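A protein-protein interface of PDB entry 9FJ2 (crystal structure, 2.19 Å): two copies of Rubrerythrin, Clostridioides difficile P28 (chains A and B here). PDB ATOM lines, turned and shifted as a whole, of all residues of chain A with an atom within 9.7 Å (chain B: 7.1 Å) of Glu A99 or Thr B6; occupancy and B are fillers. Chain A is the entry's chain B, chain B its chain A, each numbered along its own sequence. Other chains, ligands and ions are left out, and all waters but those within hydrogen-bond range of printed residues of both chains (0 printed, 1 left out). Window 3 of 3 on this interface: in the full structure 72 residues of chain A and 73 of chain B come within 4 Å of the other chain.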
ATOM      1  N   MET A  92      -2.967   2.252  25.329  1.00  0.00           N
ATOM      2  CA  MET A  92      -4.128   2.869  25.961  1.00  0.00           C
ATOM      3  C   MET A  92      -5.276   3.060  24.979  1.00  0.00           C
ATOM      4  O   MET A  92      -6.445   3.032  25.381  1.00  0.00           O
ATOM      5  CB  MET A  92      -3.737   4.212  26.578  1.00  0.00           C
ATOM      6  CG  MET A  92      -3.097   4.111  27.951  1.00  0.00           C
ATOM      7  SD  MET A  92      -2.832   5.735  28.689  1.00  0.00           S
ATOM      8  CE  MET A  92      -1.878   5.293  30.138  1.00  0.00           C
ATOM      9  N   ALA A  93      -4.970   3.257  23.696  1.00  0.00           N
ATOM     10  CA  ALA A  93      -6.025   3.492  22.716  1.00  0.00           C
ATOM     11  C   ALA A  93      -6.788   2.212  22.399  1.00  0.00           C
ATOM     12  O   ALA A  93      -8.021   2.228  22.303  1.00  0.00           O
ATOM     13  CB  ALA A  93      -5.433   4.097  21.443  1.00  0.00           C
ATOM     14  N   LYS A  94      -6.077   1.093  22.235  1.00  0.00           N
ATOM     15  CA  LYS A  94      -6.751  -0.151  21.878  1.00  0.00           C
ATOM     16  C   LYS A  94      -7.578  -0.696  23.036  1.00  0.00           C
ATOM     17  O   LYS A  94      -8.570  -1.397  22.807  1.00  0.00           O
ATOM     18  CB  LYS A  94      -5.734  -1.191  21.404  1.00  0.00           C
ATOM     19  CG  LYS A  94      -4.793  -1.707  22.481  1.00  0.00           C
ATOM     20  CD  LYS A  94      -3.760  -2.657  21.890  1.00  0.00           C
ATOM     21  CE  LYS A  94      -2.770  -3.136  22.939  1.00  0.00           C
ATOM     22  NZ  LYS A  94      -3.379  -4.126  23.869  1.00  0.00           N
ATOM     23  N   GLU A  95      -7.197  -0.387  24.278  1.00  0.00           N
ATOM     24  CA  GLU A  95      -7.994  -0.814  25.420  1.00  0.00           C
ATOM     25  C   GLU A  95      -9.240   0.044  25.596  1.00  0.00           C
ATOM     26  O   GLU A  95     -10.258  -0.445  26.101  1.00  0.00           O
ATOM     27  CB  GLU A  95      -7.149  -0.786  26.695  1.00  0.00           C
ATOM     28  CG  GLU A  95      -6.087  -1.870  26.745  1.00  0.00           C
ATOM     29  CD  GLU A  95      -5.064  -1.639  27.837  1.00  0.00           C
ATOM     30  OE1 GLU A  95      -5.221  -0.671  28.611  1.00  0.00           O
ATOM     31  OE2 GLU A  95      -4.099  -2.427  27.920  1.00  0.00           O
ATOM     32  N   ALA A  96      -9.185   1.314  25.187  1.00  0.00           N
ATOM     33  CA  ALA A  96     -10.379   2.150  25.225  1.00  0.00           C
ATOM     34  C   ALA A  96     -11.396   1.715  24.178  1.00  0.00           C
ATOM     35  O   ALA A  96     -12.606   1.827  24.407  1.00  0.00           O
ATOM     36  CB  ALA A  96     -10.005   3.619  25.025  1.00  0.00           C
ATOM     37  N   ARG A  97     -10.930   1.217  23.030  1.00  0.00           N
ATOM     38  CA  ARG A  97     -11.853   0.734  22.011  1.00  0.00           C
ATOM     39  C   ARG A  97     -12.488  -0.590  22.414  1.00  0.00           C
ATOM     40  O   ARG A  97     -13.606  -0.895  21.986  1.00  0.00           O
ATOM     41  CB  ARG A  97     -11.131   0.593  20.671  1.00  0.00           C
ATOM     42  CG  ARG A  97     -11.014   1.895  19.900  1.00  0.00           C
ATOM     43  CD  ARG A  97     -10.314   1.691  18.568  1.00  0.00           C
ATOM     44  NE  ARG A  97      -9.537   2.862  18.174  1.00  0.00           N
ATOM     45  CZ  ARG A  97     -10.058   3.973  17.662  1.00  0.00           C
ATOM     46  NH1 ARG A  97     -11.369   4.073  17.477  1.00  0.00           N
ATOM     47  NH2 ARG A  97      -9.267   4.985  17.334  1.00  0.00           N
ATOM     48  N   GLU A  98     -11.797  -1.384  23.235  1.00  0.00           N
ATOM     49  CA  GLU A  98     -12.355  -2.642  23.711  1.00  0.00           C
ATOM     50  C   GLU A  98     -13.471  -2.444  24.728  1.00  0.00           C
ATOM     51  O   GLU A  98     -14.159  -3.415  25.062  1.00  0.00           O
ATOM     52  CB  GLU A  98     -11.249  -3.511  24.314  1.00  0.00           C
ATOM     53  CG  GLU A  98     -10.285  -4.077  23.281  1.00  0.00           C
ATOM     54  CD  GLU A  98      -8.950  -4.480  23.881  1.00  0.00           C
ATOM     55  OE1 GLU A  98      -8.866  -4.606  25.123  1.00  0.00           O
ATOM     56  OE2 GLU A  98      -7.986  -4.670  23.111  1.00  0.00           O
ATOM     57  N   GLU A  99     -13.669  -1.221  25.226  1.00  0.00           N
ATOM     58  CA  GLU A  99     -14.764  -0.912  26.136  1.00  0.00           C
ATOM     59  C   GLU A  99     -15.761   0.073  25.535  1.00  0.00           C
ATOM     60  O   GLU A  99     -16.479   0.751  26.275  1.00  0.00           O
ATOM     61  CB  GLU A  99     -14.224  -0.375  27.461  1.00  0.00           C
ATOM     62  CG  GLU A  99     -14.134  -1.441  28.528  1.00  0.00           C
ATOM     63  CD  GLU A  99     -15.475  -2.108  28.762  1.00  0.00           C
ATOM     64  OE1 GLU A  99     -16.374  -1.455  29.335  1.00  0.00           O
ATOM     65  OE2 GLU A  99     -15.635  -3.279  28.357  1.00  0.00           O
ATOM     66  N   GLY A 100     -15.825   0.155  24.209  1.00  0.00           N
ATOM     67  CA  GLY A 100     -16.765   1.047  23.563  1.00  0.00           C
ATOM     68  C   GLY A 100     -16.473   2.519  23.727  1.00  0.00           C
ATOM     69  O   GLY A 100     -17.348   3.343  23.443  1.00  0.00           O
ATOM     70  N   PHE A 101     -15.274   2.880  24.182  1.00  0.00           N
ATOM     71  CA  PHE A 101     -14.883   4.284  24.311  1.00  0.00           C
ATOM     72  C   PHE A 101     -14.135   4.715  23.050  1.00  0.00           C
ATOM     73  O   PHE A 101     -12.923   4.938  23.041  1.00  0.00           O
ATOM     74  CB  PHE A 101     -14.038   4.495  25.560  1.00  0.00           C
ATOM     75  CG  PHE A 101     -14.796   4.323  26.844  1.00  0.00           C
ATOM     76  CD1 PHE A 101     -14.547   3.240  27.670  1.00  0.00           C
ATOM     77  CD2 PHE A 101     -15.754   5.247  27.227  1.00  0.00           C
ATOM     78  CE1 PHE A 101     -15.239   3.081  28.854  1.00  0.00           C
ATOM     79  CE2 PHE A 101     -16.450   5.092  28.409  1.00  0.00           C
ATOM     80  CZ  PHE A 101     -16.192   4.008  29.224  1.00  0.00           C
ATOM     81  N   ASP A 102     -14.895   4.825  21.960  1.00  0.00           N
ATOM     82  CA  ASP A 102     -14.318   5.230  20.686  1.00  0.00           C
ATOM     83  C   ASP A 102     -14.118   6.735  20.585  1.00  0.00           C
ATOM     84  O   ASP A 102     -13.270   7.182  19.806  1.00  0.00           O
ATOM     85  CB  ASP A 102     -15.199   4.748  19.531  1.00  0.00           C
ATOM     86  CG  ASP A 102     -15.548   3.276  19.643  1.00  0.00           C
ATOM     87  OD1 ASP A 102     -14.661   2.482  20.019  1.00  0.00           O
ATOM     88  OD2 ASP A 102     -16.709   2.914  19.355  1.00  0.00           O
ATOM     89  N   ASP A 103     -14.872   7.524  21.356  1.00  0.00           N
ATOM     90  CA  ASP A 103     -14.720   8.973  21.300  1.00  0.00           C
ATOM     91  C   ASP A 103     -13.391   9.415  21.901  1.00  0.00           C
ATOM     92  O   ASP A 103     -12.718  10.296  21.353  1.00  0.00           O
ATOM     93  CB  ASP A 103     -15.889   9.652  22.015  1.00  0.00           C
ATOM     94  CG  ASP A 103     -16.081   9.147  23.437  1.00  0.00           C
ATOM     95  OD1 ASP A 103     -15.765   7.968  23.704  1.00  0.00           O
ATOM     96  OD2 ASP A 103     -16.549   9.932  24.288  1.00  0.00           O
ATOM     97  N   ILE A 104     -12.993   8.815  23.025  1.00  0.00           N
ATOM     98  CA  ILE A 104     -11.743   9.201  23.670  1.00  0.00           C
ATOM     99  C   ILE A 104     -10.546   8.414  23.150  1.00  0.00           C
ATOM    100  O   ILE A 104      -9.404   8.867  23.312  1.00  0.00           O
ATOM    101  CB  ILE A 104     -11.847   9.057  25.199  1.00  0.00           C
ATOM    102  CG1 ILE A 104     -12.197   7.620  25.585  1.00  0.00           C
ATOM    103  CG2 ILE A 104     -12.882  10.023  25.757  1.00  0.00           C
ATOM    104  CD1 ILE A 104     -12.396   7.427  27.075  1.00  0.00           C
ATOM    105  N   ALA A 105     -10.769   7.250  22.535  1.00  0.00           N
ATOM    106  CA  ALA A 105      -9.670   6.547  21.882  1.00  0.00           C
ATOM    107  C   ALA A 105      -9.113   7.356  20.721  1.00  0.00           C
ATOM    108  O   ALA A 105      -7.905   7.320  20.459  1.00  0.00           O
ATOM    109  CB  ALA A 105     -10.130   5.171  21.400  1.00  0.00           C
ATOM    110  N   MET A 108      -6.838   9.950  22.349  1.00  0.00           N
ATOM    111  CA  MET A 108      -5.552   9.387  22.745  1.00  0.00           C
ATOM    112  C   MET A 108      -4.632   9.222  21.542  1.00  0.00           C
ATOM    113  O   MET A 108      -3.419   9.440  21.641  1.00  0.00           O
ATOM    114  CB  MET A 108      -5.758   8.048  23.451  1.00  0.00           C
ATOM    115  CG  MET A 108      -6.383   8.166  24.833  1.00  0.00           C
ATOM    116  SD  MET A 108      -6.822   6.566  25.541  1.00  0.00           S
ATOM    117  CE  MET A 108      -8.494   6.888  26.099  1.00  0.00           C
ATOM    118  N   LYS B   4     -16.699   4.241  35.343  1.00  0.00           N
ATOM    119  CA  LYS B   4     -16.063   3.865  36.601  1.00  0.00           C
ATOM    120  C   LYS B   4     -15.875   2.352  36.675  1.00  0.00           C
ATOM    121  O   LYS B   4     -16.720   1.589  36.205  1.00  0.00           O
ATOM    122  CB  LYS B   4     -16.891   4.359  37.790  1.00  0.00           C
ATOM    123  CG  LYS B   4     -16.262   4.074  39.143  1.00  0.00           C
ATOM    124  CD  LYS B   4     -14.978   4.869  39.308  1.00  0.00           C
ATOM    125  CE  LYS B   4     -14.308   4.582  40.641  1.00  0.00           C
ATOM    126  NZ  LYS B   4     -13.043   5.355  40.791  1.00  0.00           N
ATOM    127  N   GLY B   5     -14.761   1.923  37.266  1.00  0.00           N
ATOM    128  CA  GLY B   5     -14.438   0.516  37.365  1.00  0.00           C
ATOM    129  C   GLY B   5     -13.825  -0.086  36.122  1.00  0.00           C
ATOM    130  O   GLY B   5     -13.552  -1.293  36.110  1.00  0.00           O
ATOM    131  N   THR B   6     -13.597   0.709  35.083  1.00  0.00           N
ATOM    132  CA  THR B   6     -13.036   0.236  33.827  1.00  0.00           C
ATOM    133  C   THR B   6     -11.532   0.486  33.785  1.00  0.00           C
ATOM    134  O   THR B   6     -10.982   1.257  34.574  1.00  0.00           O
ATOM    135  CB  THR B   6     -13.710   0.929  32.639  1.00  0.00           C
ATOM    136  OG1 THR B   6     -13.653   2.350  32.820  1.00  0.00           O
ATOM    137  CG2 THR B   6     -15.164   0.500  32.528  1.00  0.00           C
ATOM    138  N   LYS B   7     -10.870  -0.189  32.842  1.00  0.00           N
ATOM    139  CA  LYS B   7      -9.436   0.008  32.662  1.00  0.00           C
ATOM    140  C   LYS B   7      -9.122   1.416  32.173  1.00  0.00           C
ATOM    141  O   LYS B   7      -8.050   1.953  32.477  1.00  0.00           O
ATOM    142  CB  LYS B   7      -8.885  -1.035  31.688  1.00  0.00           C
ATOM    143  CG  LYS B   7      -7.390  -0.934  31.435  1.00  0.00           C
ATOM    144  CD  LYS B   7      -6.597  -1.121  32.718  1.00  0.00           C
ATOM    145  CE  LYS B   7      -5.110  -0.917  32.478  1.00  0.00           C
ATOM    146  NZ  LYS B   7      -4.527  -1.997  31.633  1.00  0.00           N
ATOM    147  N   THR B   8     -10.043   2.031  31.424  1.00  0.00           N
ATOM    148  CA  THR B   8      -9.832   3.396  30.954  1.00  0.00           C
ATOM    149  C   THR B   8      -9.744   4.380  32.115  1.00  0.00           C
ATOM    150  O   THR B   8      -8.993   5.360  32.044  1.00  0.00           O
ATOM    151  CB  THR B   8     -10.953   3.796  29.990  1.00  0.00           C
ATOM    152  OG1 THR B   8     -10.974   2.889  28.881  1.00  0.00           O
ATOM    153  CG2 THR B   8     -10.737   5.204  29.465  1.00  0.00           C
ATOM    154  N   GLU B   9     -10.496   4.133  33.191  1.00  0.00           N
ATOM    155  CA  GLU B   9     -10.372   4.958  34.390  1.00  0.00           C
ATOM    156  C   GLU B   9      -8.945   4.932  34.921  1.00  0.00           C
ATOM    157  O   GLU B   9      -8.367   5.977  35.239  1.00  0.00           O
ATOM    158  CB  GLU B   9     -11.355   4.479  35.457  1.00  0.00           C
ATOM    159  CG  GLU B   9     -11.561   5.454  36.606  1.00  0.00           C
ATOM    160  CD  GLU B   9     -12.548   6.552  36.268  1.00  0.00           C
ATOM    161  OE1 GLU B   9     -13.291   6.400  35.275  1.00  0.00           O
ATOM    162  OE2 GLU B   9     -12.586   7.566  36.997  1.00  0.00           O
ATOM    163  N   LYS B  10      -8.356   3.737  35.015  1.00  0.00           N
ATOM    164  CA  LYS B  10      -6.971   3.625  35.457  1.00  0.00           C
ATOM    165  C   LYS B  10      -6.005   4.151  34.401  1.00  0.00           C
ATOM    166  O   LYS B  10      -4.956   4.709  34.745  1.00  0.00           O
ATOM    167  CB  LYS B  10      -6.661   2.168  35.808  1.00  0.00           C
ATOM    168  CG  LYS B  10      -5.190   1.850  36.030  1.00  0.00           C
ATOM    169  CD  LYS B  10      -4.935   0.353  35.910  1.00  0.00           C
ATOM    170  CE  LYS B  10      -3.511  -0.010  36.307  1.00  0.00           C
ATOM    171  NZ  LYS B  10      -3.368  -1.469  36.588  1.00  0.00           N
ATOM    172  N   ASN B  11      -6.347   4.008  33.118  1.00  0.00           N
ATOM    173  CA  ASN B  11      -5.455   4.465  32.057  1.00  0.00           C
ATOM    174  C   ASN B  11      -5.405   5.988  31.992  1.00  0.00           C
ATOM    175  O   ASN B  11      -4.320   6.583  31.969  1.00  0.00           O
ATOM    176  CB  ASN B  11      -5.890   3.873  30.715  1.00  0.00           C
ATOM    177  CG  ASN B  11      -5.283   2.503  30.456  1.00  0.00           C
ATOM    178  OD1 ASN B  11      -4.287   2.123  31.075  1.00  0.00           O
ATOM    179  ND2 ASN B  11      -5.887   1.753  29.545  1.00  0.00           N
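NZ of Lys B7 is in salt-bridge range of OE1 of Glu A95. OE1 of Glu A95 lies within hydrogen-bond range of ND2 of Asn B11 (2.7 Å). O of Asn B11 sits close to SD of Met A92, at 3.7 Å.
The backbone carbonyl oxygen (O) of Ala A96 is in hydrogen-bond range of the backbone NH (N) of Phe A101, 2.9 Å away.
Thr B8 touches Ala A96. OE1 of Glu A99 touches CG2 of Thr B6 (3.9 Å). Phe A101 touches Thr B8. CD1 of Ile A104 touches CG2 of Thr B8, at 3.7 Å.
Printed residues of chain B within 4 Å of Glu A95: Lys B7 (3.4 Å) and Asn B11 (2.7 Å). Glu A99 touches just one residue of chain B: Thr B6 (3.9 Å). Printed residues of chain B within 4 Å of Phe A101: Thr B8. No residue of chain A comes within 4 Å of Gly B5. Thr B6 touches one residue of chain A. Of the printed residues of chain A, Lys B7 touches Glu A95 (3.4 Å). Thr B8 touches just these residues of chain A: Ala A96 (3.8 Å), Phe A101 (3.8 Å) and Ile A104 (3.7 Å).
Printed residues of chain A that touch a printed residue of chain B: Met A92, Glu A95, Ala A96, Glu A99, Phe A101 and Ile A104. Hydrophobic or aromatic side chains of chain A within 4 Å of the printed part of chain B: Met A92, Phe A101 and Ile A104. Along chain A the printed residues that touch a printed residue of chain B span positions 92 to 104. Of the 8 printed residues of chain B, 4 touch a printed residue of chain A. Printed residues of chain B that touch a printed residue of chain A: Thr B6, Lys B7, Thr B8 and Asn B11.
No position is printed for both chains. Of the 7 pairs that touch across the chains among the printed residues, none has its exchanged pair printed and touching as well.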
